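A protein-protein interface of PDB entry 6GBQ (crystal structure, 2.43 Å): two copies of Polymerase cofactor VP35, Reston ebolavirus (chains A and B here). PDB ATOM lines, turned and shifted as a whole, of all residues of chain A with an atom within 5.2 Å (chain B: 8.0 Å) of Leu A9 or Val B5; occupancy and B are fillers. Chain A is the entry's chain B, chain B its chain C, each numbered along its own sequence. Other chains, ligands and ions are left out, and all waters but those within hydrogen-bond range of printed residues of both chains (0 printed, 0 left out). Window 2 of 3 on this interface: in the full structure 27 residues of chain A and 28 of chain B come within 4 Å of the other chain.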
ATOM      1  N   LEU A   2     -26.857  18.451  15.227  1.00  0.00           N
ATOM      2  CA  LEU A   2     -26.413  17.821  16.509  1.00  0.00           C
ATOM      3  C   LEU A   2     -25.217  16.889  16.293  1.00  0.00           C
ATOM      4  O   LEU A   2     -24.166  17.070  16.906  1.00  0.00           O
ATOM      5  CB  LEU A   2     -27.570  17.050  17.167  1.00  0.00           C
ATOM      6  CG  LEU A   2     -27.341  16.586  18.614  1.00  0.00           C
ATOM      7  CD1 LEU A   2     -27.397  17.765  19.575  1.00  0.00           C
ATOM      8  CD2 LEU A   2     -28.341  15.515  19.030  1.00  0.00           C
ATOM      9  N   VAL A   5     -22.284  18.777  14.657  1.00  0.00           N
ATOM     10  CA  VAL A   5     -21.647  19.724  15.588  1.00  0.00           C
ATOM     11  C   VAL A   5     -20.887  19.041  16.735  1.00  0.00           C
ATOM     12  O   VAL A   5     -19.845  19.544  17.163  1.00  0.00           O
ATOM     13  CB  VAL A   5     -22.624  20.803  16.134  1.00  0.00           C
ATOM     14  CG1 VAL A   5     -23.301  21.528  14.981  1.00  0.00           C
ATOM     15  CG2 VAL A   5     -23.654  20.238  17.101  1.00  0.00           C
ATOM     16  N   GLU A   6     -21.397  17.914  17.234  1.00  0.00           N
ATOM     17  CA  GLU A   6     -20.663  17.123  18.228  1.00  0.00           C
ATOM     18  C   GLU A   6     -19.356  16.639  17.603  1.00  0.00           C
ATOM     19  O   GLU A   6     -18.282  16.839  18.172  1.00  0.00           O
ATOM     20  CB  GLU A   6     -21.502  15.943  18.728  1.00  0.00           C
ATOM     21  CG  GLU A   6     -22.665  16.349  19.639  1.00  0.00           C
ATOM     22  CD  GLU A   6     -23.829  15.357  19.654  1.00  0.00           C
ATOM     23  OE1 GLU A   6     -23.875  14.443  18.804  1.00  0.00           O
ATOM     24  OE2 GLU A   6     -24.724  15.495  20.521  1.00  0.00           O
ATOM     25  N   ASP A   7     -19.457  16.044  16.410  1.00  0.00           N
ATOM     26  CA  ASP A   7     -18.278  15.655  15.611  1.00  0.00           C
ATOM     27  C   ASP A   7     -17.274  16.825  15.446  1.00  0.00           C
ATOM     28  O   ASP A   7     -16.064  16.612  15.543  1.00  0.00           O
ATOM     29  CB  ASP A   7     -18.686  15.102  14.217  1.00  0.00           C
ATOM     30  CG  ASP A   7     -19.305  13.682  14.268  1.00  0.00           C
ATOM     31  OD1 ASP A   7     -18.970  12.891  15.177  1.00  0.00           O
ATOM     32  OD2 ASP A   7     -20.129  13.345  13.374  1.00  0.00           O
ATOM     33  N   THR A   8     -17.786  18.036  15.202  1.00  0.00           N
ATOM     34  CA  THR A   8     -16.964  19.244  15.057  1.00  0.00           C
ATOM     35  C   THR A   8     -16.312  19.678  16.377  1.00  0.00           C
ATOM     36  O   THR A   8     -15.108  19.936  16.411  1.00  0.00           O
ATOM     37  CB  THR A   8     -17.777  20.431  14.484  1.00  0.00           C
ATOM     38  OG1 THR A   8     -18.383  20.050  13.247  1.00  0.00           O
ATOM     39  CG2 THR A   8     -16.886  21.644  14.232  1.00  0.00           C
ATOM     40  N   LEU A   9     -17.099  19.754  17.449  1.00  0.00           N
ATOM     41  CA  LEU A   9     -16.572  20.109  18.771  1.00  0.00           C
ATOM     42  C   LEU A   9     -15.436  19.183  19.240  1.00  0.00           C
ATOM     43  O   LEU A   9     -14.400  19.668  19.701  1.00  0.00           O
ATOM     44  CB  LEU A   9     -17.686  20.132  19.818  1.00  0.00           C
ATOM     45  CG  LEU A   9     -18.707  21.268  19.689  1.00  0.00           C
ATOM     46  CD1 LEU A   9     -19.970  20.925  20.459  1.00  0.00           C
ATOM     47  CD2 LEU A   9     -18.143  22.600  20.160  1.00  0.00           C
ATOM     48  N   THR A  10     -15.619  17.868  19.109  1.00  0.00           N
ATOM     49  CA  THR A  10     -14.579  16.908  19.507  1.00  0.00           C
ATOM     50  C   THR A  10     -13.345  16.982  18.602  1.00  0.00           C
ATOM     51  O   THR A  10     -12.231  16.737  19.074  1.00  0.00           O
ATOM     52  CB  THR A  10     -15.080  15.449  19.550  1.00  0.00           C
ATOM     53  OG1 THR A  10     -15.514  15.052  18.246  1.00  0.00           O
ATOM     54  CG2 THR A  10     -16.219  15.281  20.564  1.00  0.00           C
ATOM     55  N   MET A  11     -13.531  17.303  17.314  1.00  0.00           N
ATOM     56  CA  MET A  11     -12.380  17.624  16.448  1.00  0.00           C
ATOM     57  C   MET A  11     -11.624  18.817  17.021  1.00  0.00           C
ATOM     58  O   MET A  11     -10.407  18.796  17.061  1.00  0.00           O
ATOM     59  CB  MET A  11     -12.760  17.933  14.984  1.00  0.00           C
ATOM     60  CG  MET A  11     -11.658  18.727  14.267  1.00  0.00           C
ATOM     61  SD  MET A  11     -11.772  18.992  12.497  1.00  0.00           S
ATOM     62  CE  MET A  11     -10.193  19.799  12.214  1.00  0.00           C
ATOM     63  N   LEU A  12     -12.352  19.859  17.415  1.00  0.00           N
ATOM     64  CA  LEU A  12     -11.747  21.081  17.943  1.00  0.00           C
ATOM     65  C   LEU A  12     -10.966  20.842  19.233  1.00  0.00           C
ATOM     66  O   LEU A  12      -9.849  21.343  19.372  1.00  0.00           O
ATOM     67  CB  LEU A  12     -12.798  22.183  18.145  1.00  0.00           C
ATOM     68  CG  LEU A  12     -13.297  22.849  16.856  1.00  0.00           C
ATOM     69  CD1 LEU A  12     -14.490  23.749  17.150  1.00  0.00           C
ATOM     70  CD2 LEU A  12     -12.168  23.616  16.166  1.00  0.00           C
ATOM     71  N   VAL A  13     -11.538  20.057  20.144  1.00  0.00           N
ATOM     72  CA  VAL A  13     -10.835  19.630  21.365  1.00  0.00           C
ATOM     73  C   VAL A  13      -9.548  18.871  21.011  1.00  0.00           C
ATOM     74  O   VAL A  13      -8.496  19.092  21.615  1.00  0.00           O
ATOM     75  CB  VAL A  13     -11.738  18.759  22.269  1.00  0.00           C
ATOM     76  CG1 VAL A  13     -10.940  18.121  23.406  1.00  0.00           C
ATOM     77  CG2 VAL A  13     -12.882  19.594  22.835  1.00  0.00           C
ATOM     78  N   ASN A  14      -9.640  17.993  20.023  1.00  0.00           N
ATOM     79  CA  ASN A  14      -8.481  17.268  19.541  1.00  0.00           C
ATOM     80  C   ASN A  14      -7.484  18.210  18.854  1.00  0.00           C
ATOM     81  O   ASN A  14      -6.290  18.164  19.153  1.00  0.00           O
ATOM     82  CB  ASN A  14      -8.919  16.143  18.598  1.00  0.00           C
ATOM     83  CG  ASN A  14      -7.785  15.222  18.209  1.00  0.00           C
ATOM     84  OD1 ASN A  14      -6.894  14.942  19.011  1.00  0.00           O
ATOM     85  ND2 ASN A  14      -7.818  14.730  16.974  1.00  0.00           N
ATOM     86  N   LEU B   2     -28.114  17.747  23.686  1.00  0.00           N
ATOM     87  CA  LEU B   2     -27.527  18.989  24.279  1.00  0.00           C
ATOM     88  C   LEU B   2     -26.411  18.692  25.290  1.00  0.00           C
ATOM     89  O   LEU B   2     -25.397  19.395  25.313  1.00  0.00           O
ATOM     90  CB  LEU B   2     -28.630  19.840  24.931  1.00  0.00           C
ATOM     91  CG  LEU B   2     -28.436  21.361  25.018  1.00  0.00           C
ATOM     92  CD1 LEU B   2     -28.285  21.997  23.641  1.00  0.00           C
ATOM     93  CD2 LEU B   2     -29.604  21.989  25.767  1.00  0.00           C
ATOM     94  N   LYS B   3     -26.592  17.658  26.113  1.00  0.00           N
ATOM     95  CA  LYS B   3     -25.638  17.334  27.185  1.00  0.00           C
ATOM     96  C   LYS B   3     -24.245  16.949  26.669  1.00  0.00           C
ATOM     97  O   LYS B   3     -23.240  17.390  27.228  1.00  0.00           O
ATOM     98  CB  LYS B   3     -26.189  16.228  28.090  1.00  0.00           C
ATOM     99  CG  LYS B   3     -27.398  16.661  28.902  1.00  0.00           C
ATOM    100  CD  LYS B   3     -28.045  15.482  29.611  1.00  0.00           C
ATOM    101  CE  LYS B   3     -29.392  15.870  30.202  1.00  0.00           C
ATOM    102  NZ  LYS B   3     -29.988  14.762  30.996  1.00  0.00           N
ATOM    103  N   LYS B   4     -24.192  16.134  25.615  1.00  0.00           N
ATOM    104  CA  LYS B   4     -22.918  15.798  24.961  1.00  0.00           C
ATOM    105  C   LYS B   4     -22.256  17.013  24.298  1.00  0.00           C
ATOM    106  O   LYS B   4     -21.024  17.089  24.243  1.00  0.00           O
ATOM    107  CB  LYS B   4     -23.085  14.661  23.944  1.00  0.00           C
ATOM    108  CG  LYS B   4     -23.252  13.295  24.589  1.00  0.00           C
ATOM    109  CD  LYS B   4     -23.270  12.172  23.561  1.00  0.00           C
ATOM    110  CE  LYS B   4     -23.372  10.807  24.228  1.00  0.00           C
ATOM    111  NZ  LYS B   4     -23.355   9.698  23.234  1.00  0.00           N
ATOM    112  N   VAL B   5     -23.064  17.952  23.801  1.00  0.00           N
ATOM    113  CA  VAL B   5     -22.549  19.231  23.296  1.00  0.00           C
ATOM    114  C   VAL B   5     -21.994  20.071  24.454  1.00  0.00           C
ATOM    115  O   VAL B   5     -20.875  20.581  24.361  1.00  0.00           O
ATOM    116  CB  VAL B   5     -23.619  20.019  22.495  1.00  0.00           C
ATOM    117  CG1 VAL B   5     -23.186  21.461  22.229  1.00  0.00           C
ATOM    118  CG2 VAL B   5     -23.918  19.307  21.181  1.00  0.00           C
ATOM    119  N   GLU B   6     -22.767  20.201  25.533  1.00  0.00           N
ATOM    120  CA  GLU B   6     -22.360  21.025  26.684  1.00  0.00           C
ATOM    121  C   GLU B   6     -21.109  20.516  27.420  1.00  0.00           C
ATOM    122  O   GLU B   6     -20.324  21.321  27.925  1.00  0.00           O
ATOM    123  CB  GLU B   6     -23.523  21.225  27.670  1.00  0.00           C
ATOM    124  CG  GLU B   6     -24.578  22.211  27.174  1.00  0.00           C
ATOM    125  CD  GLU B   6     -25.214  23.019  28.292  1.00  0.00           C
ATOM    126  OE1 GLU B   6     -26.208  22.536  28.882  1.00  0.00           O
ATOM    127  OE2 GLU B   6     -24.729  24.144  28.562  1.00  0.00           O
ATOM    128  N   ASP B   7     -20.928  19.196  27.470  1.00  0.00           N
ATOM    129  CA  ASP B   7     -19.714  18.601  28.035  1.00  0.00           C
ATOM    130  C   ASP B   7     -18.501  18.813  27.132  1.00  0.00           C
ATOM    131  O   ASP B   7     -17.421  19.136  27.622  1.00  0.00           O
ATOM    132  CB  ASP B   7     -19.906  17.103  28.303  1.00  0.00           C
ATOM    133  CG  ASP B   7     -20.938  16.827  29.383  1.00  0.00           C
ATOM    134  OD1 ASP B   7     -21.139  17.688  30.264  1.00  0.00           O
ATOM    135  OD2 ASP B   7     -21.552  15.740  29.354  1.00  0.00           O
ATOM    136  N   THR B   8     -18.672  18.626  25.825  1.00  0.00           N
ATOM    137  CA  THR B   8     -17.567  18.800  24.875  1.00  0.00           C
ATOM    138  C   THR B   8     -17.164  20.285  24.778  1.00  0.00           C
ATOM    139  O   THR B   8     -15.997  20.610  24.529  1.00  0.00           O
ATOM    140  CB  THR B   8     -17.911  18.202  23.491  1.00  0.00           C
ATOM    141  OG1 THR B   8     -18.388  16.860  23.659  1.00  0.00           O
ATOM    142  CG2 THR B   8     -16.686  18.155  22.576  1.00  0.00           C
ATOM    143  N   LEU B   9     -18.131  21.173  24.992  1.00  0.00           N
ATOM    144  CA  LEU B   9     -17.870  22.606  25.064  1.00  0.00           C
ATOM    145  C   LEU B   9     -17.047  22.983  26.300  1.00  0.00           C
ATOM    146  O   LEU B   9     -16.156  23.834  26.223  1.00  0.00           O
ATOM    147  CB  LEU B   9     -19.194  23.367  25.069  1.00  0.00           C
ATOM    148  CG  LEU B   9     -19.170  24.889  25.039  1.00  0.00           C
ATOM    149  CD1 LEU B   9     -18.338  25.413  23.880  1.00  0.00           C
ATOM    150  CD2 LEU B   9     -20.607  25.384  24.949  1.00  0.00           C
ATOM    151  N   THR B  10     -17.368  22.364  27.434  1.00  0.00           N
ATOM    152  CA  THR B  10     -16.608  22.551  28.671  1.00  0.00           C
ATOM    153  C   THR B  10     -15.149  22.081  28.508  1.00  0.00           C
ATOM    154  O   THR B  10     -14.230  22.771  28.946  1.00  0.00           O
ATOM    155  CB  THR B  10     -17.313  21.872  29.874  1.00  0.00           C
ATOM    156  OG1 THR B  10     -18.395  22.705  30.309  1.00  0.00           O
ATOM    157  CG2 THR B  10     -16.360  21.660  31.063  1.00  0.00           C
ATOM    158  N   MET B  11     -14.954  20.924  27.873  1.00  0.00           N
ATOM    159  CA  MET B  11     -13.618  20.431  27.535  1.00  0.00           C
ATOM    160  C   MET B  11     -12.866  21.431  26.647  1.00  0.00           C
ATOM    161  O   MET B  11     -11.658  21.642  26.810  1.00  0.00           O
ATOM    162  CB  MET B  11     -13.702  19.093  26.796  1.00  0.00           C
ATOM    163  CG  MET B  11     -14.211  17.910  27.604  1.00  0.00           C
ATOM    164  SD  MET B  11     -14.211  16.386  26.614  1.00  0.00           S
ATOM    165  CE  MET B  11     -12.452  16.023  26.603  1.00  0.00           C
ATOM    166  N   LEU B  12     -13.582  22.031  25.700  1.00  0.00           N
ATOM    167  CA  LEU B  12     -13.010  23.008  24.777  1.00  0.00           C
ATOM    168  C   LEU B  12     -12.646  24.321  25.469  1.00  0.00           C
ATOM    169  O   LEU B  12     -11.659  24.971  25.117  1.00  0.00           O
ATOM    170  CB  LEU B  12     -13.995  23.279  23.641  1.00  0.00           C
ATOM    171  CG  LEU B  12     -13.520  24.140  22.476  1.00  0.00           C
ATOM    172  CD1 LEU B  12     -12.289  23.525  21.812  1.00  0.00           C
ATOM    173  CD2 LEU B  12     -14.665  24.299  21.479  1.00  0.00           C
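Of the 11 printed residues of chain A, 5 touch a printed residue of chain B.
Printed residues of chain A that touch a printed residue of chain B: Glu A6, Leu A9, Thr A10, Leu A12 and Val A13.
Hydrophobic or aromatic side chains of chain B within 4 Å of the printed part of chain A: Val B5 and Leu B12.
Among the printed residues, no Asp or Glu carboxylate lies within 4 Å of a Lys or Arg side-chain nitrogen of the other chain.
OG1 of Thr A10 is in hydrogen-bond range of O of Asp A7.
O of Lys B4 lies within hydrogen-bond range of OG1 of Thr B8 (2.7 Å).
O of Glu A6 lies within hydrogen-bond range of OG1 of Thr A10.
Lys B4 touches Glu A6.
Val B5 touches Glu A6 (CG2 to CG, 3.6 Å).
Leu A9 touches Val B5 (CD1 to CG1, 3.7 Å).
Leu A9 touches Thr B8 (CB to CG2, 3.5 Å).
Thr B8 touches Thr A10.
Leu A12 touches Leu B12 (CB to CD1, 3.9 Å).
Thr B8 touches Val A13 (O to CG2, 3.7 Å).
Val A13 touches Leu B12 (CG2 to N, 3.8 Å).
Glu A6 touches Val B5, but with the chains exchanged Val A5 does not touch Glu B6 (8.5 Å).
Leu A9 touches Val B5, but with the chains exchanged Val A5 does not touch Leu B9 (8.2 Å).
Leu A9 touches Thr B8, but with the chains exchanged Thr A8 does not touch Leu B9 (8.9 Å).
Thr A10 touches Thr B8, but with the chains exchanged Thr A8 does not touch Thr B10 (11.4 Å).
9 positions are printed for both chains.
Printed residues of chain B within 4 Å of Glu A6: Lys B4 (3.9 Å) and Val B5 (3.6 Å).
Thr A8 touches none of the printed residues of chain B.
Of chain B, only Val B5 and Thr B8 come within 4 Å of Leu A9.
Leu B2 touches none of the printed residues of chain A.
Of the printed residues of chain A, Lys B4 touches Glu A6.
Val B5 touches two residues of chain A.
The nearest residue of chain B that does not touch Leu A9 is Leu B12 (4.1 Å).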
